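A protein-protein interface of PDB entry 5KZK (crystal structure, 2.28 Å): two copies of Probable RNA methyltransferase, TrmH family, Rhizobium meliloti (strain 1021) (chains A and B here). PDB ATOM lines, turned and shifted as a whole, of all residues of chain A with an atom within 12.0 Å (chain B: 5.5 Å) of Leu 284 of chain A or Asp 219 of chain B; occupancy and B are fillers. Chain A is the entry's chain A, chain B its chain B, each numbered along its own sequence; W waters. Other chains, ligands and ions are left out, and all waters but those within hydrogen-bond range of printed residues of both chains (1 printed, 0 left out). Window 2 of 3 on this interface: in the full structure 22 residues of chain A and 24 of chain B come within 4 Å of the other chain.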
ATOM      1  N   ALA A 157      -2.211  16.395 -14.500  1.00  0.00           N
ATOM      2  CA  ALA A 157      -2.239  17.335 -15.664  1.00  0.00           C
ATOM      3  C   ALA A 157      -3.546  17.460 -16.407  1.00  0.00           C
ATOM      4  O   ALA A 157      -3.845  18.525 -16.826  1.00  0.00           O
ATOM      5  CB  ALA A 157      -1.191  17.028 -16.681  1.00  0.00           C
ATOM      6  N   ALA A 158      -4.246  16.390 -16.710  1.00  0.00           N
ATOM      7  CA  ALA A 158      -5.465  16.478 -17.426  1.00  0.00           C
ATOM      8  C   ALA A 158      -6.662  16.985 -16.584  1.00  0.00           C
ATOM      9  O   ALA A 158      -7.626  17.400 -17.137  1.00  0.00           O
ATOM     10  CB  ALA A 158      -5.847  15.154 -18.040  1.00  0.00           C
ATOM     11  N   PHE A 275      -7.037  12.796 -22.529  1.00  0.00           N
ATOM     12  CA  PHE A 275      -7.104  14.008 -23.368  1.00  0.00           C
ATOM     13  C   PHE A 275      -8.294  14.058 -24.375  1.00  0.00           C
ATOM     14  O   PHE A 275      -8.683  15.093 -24.869  1.00  0.00           O
ATOM     15  CB  PHE A 275      -5.734  14.436 -23.941  1.00  0.00           C
ATOM     16  CG  PHE A 275      -4.833  15.094 -22.865  1.00  0.00           C
ATOM     17  CD1 PHE A 275      -4.030  14.335 -21.996  1.00  0.00           C
ATOM     18  CD2 PHE A 275      -4.826  16.458 -22.683  1.00  0.00           C
ATOM     19  CE1 PHE A 275      -3.370  14.932 -20.922  1.00  0.00           C
ATOM     20  CE2 PHE A 275      -4.132  17.039 -21.674  1.00  0.00           C
ATOM     21  CZ  PHE A 275      -3.413  16.291 -20.749  1.00  0.00           C
ATOM     22  N   GLU A 276      -8.840  12.933 -24.733  1.00  0.00           N
ATOM     23  CA  GLU A 276     -10.042  12.885 -25.496  1.00  0.00           C
ATOM     24  C   GLU A 276     -11.261  13.046 -24.576  1.00  0.00           C
ATOM     25  O   GLU A 276     -12.196  13.778 -24.901  1.00  0.00           O
ATOM     26  CB  GLU A 276     -10.126  11.581 -26.230  1.00  0.00           C
ATOM     27  CG  GLU A 276     -11.217  11.630 -27.308  1.00  0.00           C
ATOM     28  CD  GLU A 276     -10.833  12.554 -28.493  1.00  0.00           C
ATOM     29  OE1 GLU A 276      -9.624  12.655 -28.819  1.00  0.00           O
ATOM     30  OE2 GLU A 276     -11.756  13.099 -29.199  1.00  0.00           O
ATOM     31  N   ARG A 278     -11.563  14.578 -21.816  1.00  0.00           N
ATOM     32  CA  ARG A 278     -11.582  15.916 -21.295  1.00  0.00           C
ATOM     33  C   ARG A 278     -11.306  16.949 -22.356  1.00  0.00           C
ATOM     34  O   ARG A 278     -11.085  18.134 -22.058  1.00  0.00           O
ATOM     35  CB  ARG A 278     -10.546  16.018 -20.170  1.00  0.00           C
ATOM     36  CG  ARG A 278     -10.990  15.134 -19.001  1.00  0.00           C
ATOM     37  CD  ARG A 278     -10.295  15.409 -17.746  1.00  0.00           C
ATOM     38  NE  ARG A 278     -10.600  16.721 -17.180  1.00  0.00           N
ATOM     39  CZ  ARG A 278     -11.745  17.030 -16.508  1.00  0.00           C
ATOM     40  NH1 ARG A 278     -12.697  16.129 -16.328  1.00  0.00           N
ATOM     41  NH2 ARG A 278     -11.936  18.238 -16.024  1.00  0.00           N
ATOM     42  N   ARG A 279     -11.403  16.523 -23.609  1.00  0.00           N
ATOM     43  CA  ARG A 279     -11.118  17.380 -24.697  1.00  0.00           C
ATOM     44  C   ARG A 279     -12.025  18.634 -24.667  1.00  0.00           C
ATOM     45  O   ARG A 279     -11.538  19.747 -24.872  1.00  0.00           O
ATOM     46  CB  ARG A 279     -11.307  16.688 -25.990  1.00  0.00           C
ATOM     47  CG  ARG A 279     -10.862  17.527 -27.199  1.00  0.00           C
ATOM     48  CD  ARG A 279     -11.163  16.785 -28.446  1.00  0.00           C
ATOM     49  NE  ARG A 279     -10.763  17.392 -29.722  1.00  0.00           N
ATOM     50  CZ  ARG A 279      -9.561  17.278 -30.337  1.00  0.00           C
ATOM     51  NH1 ARG A 279      -9.363  17.857 -31.572  1.00  0.00           N
ATOM     52  NH2 ARG A 279      -8.574  16.616 -29.781  1.00  0.00           N
ATOM     53  N   HIS A 280     -13.323  18.409 -24.486  1.00  0.00           N
ATOM     54  CA  HIS A 280     -14.309  19.488 -24.396  1.00  0.00           C
ATOM     55  C   HIS A 280     -14.217  20.326 -23.125  1.00  0.00           C
ATOM     56  O   HIS A 280     -14.937  21.239 -23.007  1.00  0.00           O
ATOM     57  CB  HIS A 280     -15.730  18.879 -24.531  1.00  0.00           C
ATOM     58  CG  HIS A 280     -16.222  18.199 -23.298  1.00  0.00           C
ATOM     59  ND1 HIS A 280     -15.768  16.956 -22.876  1.00  0.00           N
ATOM     60  CD2 HIS A 280     -17.137  18.593 -22.387  1.00  0.00           C
ATOM     61  CE1 HIS A 280     -16.365  16.620 -21.752  1.00  0.00           C
ATOM     62  NE2 HIS A 280     -17.196  17.609 -21.428  1.00  0.00           N
ATOM     63  N   LEU A 281     -13.358  19.988 -22.174  1.00  0.00           N
ATOM     64  CA  LEU A 281     -13.188  20.675 -20.906  1.00  0.00           C
ATOM     65  C   LEU A 281     -11.839  21.462 -20.681  1.00  0.00           C
ATOM     66  O   LEU A 281     -11.691  22.194 -19.700  1.00  0.00           O
ATOM     67  CB  LEU A 281     -13.320  19.629 -19.791  1.00  0.00           C
ATOM     68  CG  LEU A 281     -14.749  19.113 -19.525  1.00  0.00           C
ATOM     69  CD1 LEU A 281     -14.786  17.918 -18.617  1.00  0.00           C
ATOM     70  CD2 LEU A 281     -15.638  20.209 -18.921  1.00  0.00           C
ATOM     71  N   LEU A 282     -10.871  21.260 -21.554  1.00  0.00           N
ATOM     72  CA  LEU A 282      -9.542  21.800 -21.424  1.00  0.00           C
ATOM     73  C   LEU A 282      -9.431  22.849 -22.488  1.00  0.00           C
ATOM     74  O   LEU A 282      -9.710  22.570 -23.638  1.00  0.00           O
ATOM     75  CB  LEU A 282      -8.479  20.720 -21.721  1.00  0.00           C
ATOM     76  CG  LEU A 282      -8.378  19.655 -20.681  1.00  0.00           C
ATOM     77  CD1 LEU A 282      -7.524  18.449 -21.128  1.00  0.00           C
ATOM     78  CD2 LEU A 282      -7.913  20.229 -19.370  1.00  0.00           C
ATOM     79  N   SER A 283      -9.012  24.045 -22.122  1.00  0.00           N
ATOM     80  CA  SER A 283      -8.806  25.153 -23.083  1.00  0.00           C
ATOM     81  C   SER A 283      -7.619  26.009 -22.627  1.00  0.00           C
ATOM     82  O   SER A 283      -7.114  25.881 -21.492  1.00  0.00           O
ATOM     83  CB  SER A 283     -10.080  26.004 -23.243  1.00  0.00           C
ATOM     84  OG  SER A 283     -10.566  26.243 -21.942  1.00  0.00           O
ATOM     85  N   LEU A 284      -7.164  26.862 -23.525  1.00  0.00           N
ATOM     86  CA  LEU A 284      -5.915  27.594 -23.275  1.00  0.00           C
ATOM     87  C   LEU A 284      -6.104  28.890 -22.447  1.00  0.00           C
ATOM     88  O   LEU A 284      -7.070  29.639 -22.629  1.00  0.00           O
ATOM     89  CB  LEU A 284      -5.191  27.840 -24.615  1.00  0.00           C
ATOM     90  CG  LEU A 284      -3.652  27.755 -24.511  1.00  0.00           C
ATOM     91  CD1 LEU A 284      -3.172  26.383 -24.039  1.00  0.00           C
ATOM     92  CD2 LEU A 284      -2.920  28.138 -25.812  1.00  0.00           C
ATOM     93  N   SER B 217       3.067  29.998 -28.351  1.00  0.00           N
ATOM     94  CA  SER B 217       2.344  28.760 -28.746  1.00  0.00           C
ATOM     95  C   SER B 217       0.853  28.959 -28.940  1.00  0.00           C
ATOM     96  O   SER B 217       0.332  29.939 -28.526  1.00  0.00           O
ATOM     97  CB  SER B 217       2.600  27.632 -27.767  1.00  0.00           C
ATOM     98  OG  SER B 217       2.158  27.921 -26.475  1.00  0.00           O
ATOM     99  N   VAL B 218       0.225  28.066 -29.693  1.00  0.00           N
ATOM    100  CA  VAL B 218      -1.232  27.980 -29.834  1.00  0.00           C
ATOM    101  C   VAL B 218      -1.655  26.559 -29.331  1.00  0.00           C
ATOM    102  O   VAL B 218      -0.884  25.588 -29.285  1.00  0.00           O
ATOM    103  CB  VAL B 218      -1.746  28.251 -31.309  1.00  0.00           C
ATOM    104  CG1 VAL B 218      -1.530  29.738 -31.756  1.00  0.00           C
ATOM    105  CG2 VAL B 218      -1.121  27.284 -32.370  1.00  0.00           C
ATOM    106  N   ASP B 219      -2.923  26.457 -29.050  1.00  0.00           N
ATOM    107  CA  ASP B 219      -3.566  25.230 -28.758  1.00  0.00           C
ATOM    108  C   ASP B 219      -3.302  24.226 -29.886  1.00  0.00           C
ATOM    109  O   ASP B 219      -3.606  24.494 -31.002  1.00  0.00           O
ATOM    110  CB  ASP B 219      -5.046  25.489 -28.504  1.00  0.00           C
ATOM    111  CG  ASP B 219      -5.841  24.222 -28.211  1.00  0.00           C
ATOM    112  OD1 ASP B 219      -5.597  23.135 -28.766  1.00  0.00           O
ATOM    113  OD2 ASP B 219      -6.750  24.338 -27.378  1.00  0.00           O
ATOM    114  N   TYR B 220      -2.647  23.104 -29.551  1.00  0.00           N
ATOM    115  CA  TYR B 220      -2.309  22.031 -30.526  1.00  0.00           C
ATOM    116  C   TYR B 220      -3.480  21.561 -31.416  1.00  0.00           C
ATOM    117  O   TYR B 220      -3.290  21.068 -32.602  1.00  0.00           O
ATOM    118  CB  TYR B 220      -1.672  20.839 -29.756  1.00  0.00           C
ATOM    119  CG  TYR B 220      -2.649  19.879 -29.020  1.00  0.00           C
ATOM    120  CD1 TYR B 220      -3.324  20.259 -27.900  1.00  0.00           C
ATOM    121  CD2 TYR B 220      -2.826  18.567 -29.435  1.00  0.00           C
ATOM    122  CE1 TYR B 220      -4.208  19.399 -27.244  1.00  0.00           C
ATOM    123  CE2 TYR B 220      -3.688  17.676 -28.770  1.00  0.00           C
ATOM    124  CZ  TYR B 220      -4.381  18.081 -27.692  1.00  0.00           C
ATOM    125  OH  TYR B 220      -5.255  17.244 -26.966  1.00  0.00           O
ATOM    126  N   ARG B 221      -4.685  21.685 -30.853  1.00  0.00           N
ATOM    127  CA  ARG B 221      -5.882  21.312 -31.559  1.00  0.00           C
ATOM    128  C   ARG B 221      -6.392  22.326 -32.642  1.00  0.00           C
ATOM    129  O   ARG B 221      -7.317  22.037 -33.377  1.00  0.00           O
ATOM    130  CB  ARG B 221      -7.029  20.972 -30.585  1.00  0.00           C
ATOM    131  CG  ARG B 221      -6.691  19.825 -29.685  1.00  0.00           C
ATOM    132  CD  ARG B 221      -7.454  19.705 -28.346  1.00  0.00           C
ATOM    133  NE  ARG B 221      -7.532  20.976 -27.635  1.00  0.00           N
ATOM    134  CZ  ARG B 221      -8.294  21.220 -26.551  1.00  0.00           C
ATOM    135  NH1 ARG B 221      -9.042  20.248 -25.980  1.00  0.00           N
ATOM    136  NH2 ARG B 221      -8.312  22.472 -26.050  1.00  0.00           N
ATOM    137  N   THR B 222      -5.781  23.490 -32.758  1.00  0.00           N
ATOM    138  CA  THR B 222      -6.231  24.481 -33.752  1.00  0.00           C
ATOM    139  C   THR B 222      -5.215  24.555 -34.878  1.00  0.00           C
ATOM    140  O   THR B 222      -5.402  25.373 -35.801  1.00  0.00           O
ATOM    141  CB  THR B 222      -6.382  25.905 -33.139  1.00  0.00           C
ATOM    142  OG1 THR B 222      -5.110  26.314 -32.666  1.00  0.00           O
ATOM    143  CG2 THR B 222      -7.325  25.909 -31.952  1.00  0.00           C
ATOM    144  N   ILE B 223      -4.140  23.766 -34.835  1.00  0.00           N
ATOM    145  CA  ILE B 223      -3.088  23.897 -35.881  1.00  0.00           C
ATOM    146  C   ILE B 223      -3.500  23.135 -37.137  1.00  0.00           C
ATOM    147  O   ILE B 223      -4.291  22.209 -37.078  1.00  0.00           O
ATOM    148  CB  ILE B 223      -1.718  23.368 -35.367  1.00  0.00           C
ATOM    149  CG1 ILE B 223      -1.160  24.331 -34.387  1.00  0.00           C
ATOM    150  CG2 ILE B 223      -0.664  23.067 -36.463  1.00  0.00           C
ATOM    151  CD1 ILE B 223      -0.258  23.711 -33.360  1.00  0.00           C
ATOM    152  N   ALA B 253       3.231  24.754 -30.704  1.00  0.00           N
ATOM    153  CA  ALA B 253       2.083  24.122 -30.109  1.00  0.00           C
ATOM    154  C   ALA B 253       2.205  23.957 -28.614  1.00  0.00           C
ATOM    155  O   ALA B 253       3.306  23.772 -28.021  1.00  0.00           O
ATOM    156  CB  ALA B 253       1.822  22.770 -30.749  1.00  0.00           C
ATOM    157  N   ARG B 254       1.056  23.909 -28.036  1.00  0.00           N
ATOM    158  CA  ARG B 254       0.984  23.528 -26.677  1.00  0.00           C
ATOM    159  C   ARG B 254      -0.319  22.752 -26.343  1.00  0.00           C
ATOM    160  O   ARG B 254      -1.385  22.971 -26.906  1.00  0.00           O
ATOM    161  CB  ARG B 254       1.167  24.849 -25.972  1.00  0.00           C
ATOM    162  CG  ARG B 254       0.790  24.988 -24.565  1.00  0.00           C
ATOM    163  CD  ARG B 254       0.354  26.503 -24.309  1.00  0.00           C
ATOM    164  NE  ARG B 254       0.006  26.614 -22.889  1.00  0.00           N
ATOM    165  CZ  ARG B 254      -0.198  27.725 -22.175  1.00  0.00           C
ATOM    166  NH1 ARG B 254      -0.131  28.942 -22.718  1.00  0.00           N
ATOM    167  NH2 ARG B 254      -0.482  27.575 -20.881  1.00  0.00           N
ATOM    168  N   ILE B 255      -0.240  21.941 -25.335  1.00  0.00           N
ATOM    169  CA  ILE B 255      -1.341  21.131 -24.840  1.00  0.00           C
ATOM    170  C   ILE B 255      -1.953  21.712 -23.575  1.00  0.00           C
ATOM    171  O   ILE B 255      -1.295  21.724 -22.530  1.00  0.00           O
ATOM    172  CB  ILE B 255      -0.893  19.671 -24.562  1.00  0.00           C
ATOM    173  CG1 ILE B 255      -0.474  18.991 -25.880  1.00  0.00           C
ATOM    174  CG2 ILE B 255      -2.093  18.902 -23.967  1.00  0.00           C
ATOM    175  CD1 ILE B 255       0.547  17.940 -25.643  1.00  0.00           C
ATOM    176  N   PRO B 256      -3.218  22.173 -23.650  1.00  0.00           N
ATOM    177  CA  PRO B 256      -3.871  22.796 -22.473  1.00  0.00           C
ATOM    178  C   PRO B 256      -3.953  21.787 -21.428  1.00  0.00           C
ATOM    179  O   PRO B 256      -4.179  20.649 -21.752  1.00  0.00           O
ATOM    180  CB  PRO B 256      -5.293  23.132 -22.971  1.00  0.00           C
ATOM    181  CG  PRO B 256      -5.063  23.343 -24.418  1.00  0.00           C
ATOM    182  CD  PRO B 256      -4.047  22.316 -24.839  1.00  0.00           C
HETATM  183  O   HOH W   1      -7.457  17.648 -25.598  1.00  0.00           O
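The backbone NH of Tyr 220 of chain B sits at hydrogen-bond distance from the backbone carbonyl oxygen of Arg 254 of chain B.
The backbone carbonyl oxygen (O) of Val 218 of chain B lies within hydrogen-bond range of the backbone NH (N) of Arg 254 of chain B (2.9 Å).
OD2 of Asp 219 of chain B lies within salt-bridge range of NH2 of Arg 221 of chain B (2.8 Å).
O of Asp 219 of chain B lies within hydrogen-bond range of OG1 of Thr 222 of chain B (2.9 Å).
Among the printed residues, merely in contact across the chains: Phe 275 of chain A with Ile 255 of chain B, Phe 275 of chain A with Pro 256 of chain B, Ser 283 of chain A with Pro 256 of chain B, Leu 284 of chain A with Asp 219 of chain B, Leu 284 of chain A with Arg 254 of chain B and Leu 284 of chain A with Pro 256 of chain B.
O of Leu 282 of chain A lies within hydrogen-bond range of NH2 of Arg 221 of chain B, 2.8 Å away.
The guanidinium group (NH1) of Arg 221 of chain B lies within hydrogen-bond range of the backbone carbonyl oxygen (O) of Arg 279 of chain A, at 2.8 Å.
Hydrophobic or aromatic side chains of chain B within 4 Å of the printed part of chain A: Ile 255 and Pro 256.
Along chain B the printed residues that touch a printed residue of chain A span positions 219 to 256.
Hydrophobic or aromatic side chains of chain A within 4 Å of the printed part of chain B: Phe 275 and Leu 284.
Among the printed residues, 8 pairs touch across the chains.
Printed residues of chain B within 4 Å of Leu 284 of chain A: Asp 219 (3.6 Å), Arg 254 (3.4 Å) and Pro 256 (3.6 Å).
Printed residues of chain A within 4 Å of Asp 219 of chain B: Leu 284.
No residue of chain A comes within 4 Å of Ser 217 of chain B.
No residue of chain A comes within 4 Å of Val 218 of chain B.
No residue of chain A comes within 4 Å of Tyr 220 of chain B.
Of chain A, only Arg 279 and Leu 282 come within 4 Å of Arg 221 of chain B.
No residue of chain A comes within 4 Å of Thr 222 of chain B.
No residue of chain A comes within 4 Å of Ile 223 of chain B.
No residue of chain A comes within 4 Å of Ala 253 of chain B.
Arg 254 of chain B touches just one residue of chain A: Leu 284.
Pro 256 of chain B touches three residues of chain A.
Of the printed residues of chain B, Leu 282 of chain A touches Arg 221.
Printed residues of chain A within 4 Å of Ile 255 of chain B: Phe 275 (3.6 Å).
Of the printed residues of chain B, Arg 279 of chain A touches Arg 221.
Printed residues of chain B within 4 Å of Ser 283 of chain A: Pro 256 (3.6 Å).
Ala 157 of chain A touches none of the printed residues of chain B.
Ala 158 of chain A touches none of the printed residues of chain B.
The nearest residue of chain B that does not touch Leu 284 of chain A is Val 218 of chain B (4.1 Å).
No position is printed for both chains.
Of the 8 pairs that touch across the chains among the printed residues, none has its exchanged pair printed and touching as well.
Water W1 lies within hydrogen-bond range of OH of Tyr 220 of chain B (2.6 Å), O of Phe 275 of chain A (2.9 Å) and NH1 of Arg 221 of chain B (3.1 Å).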
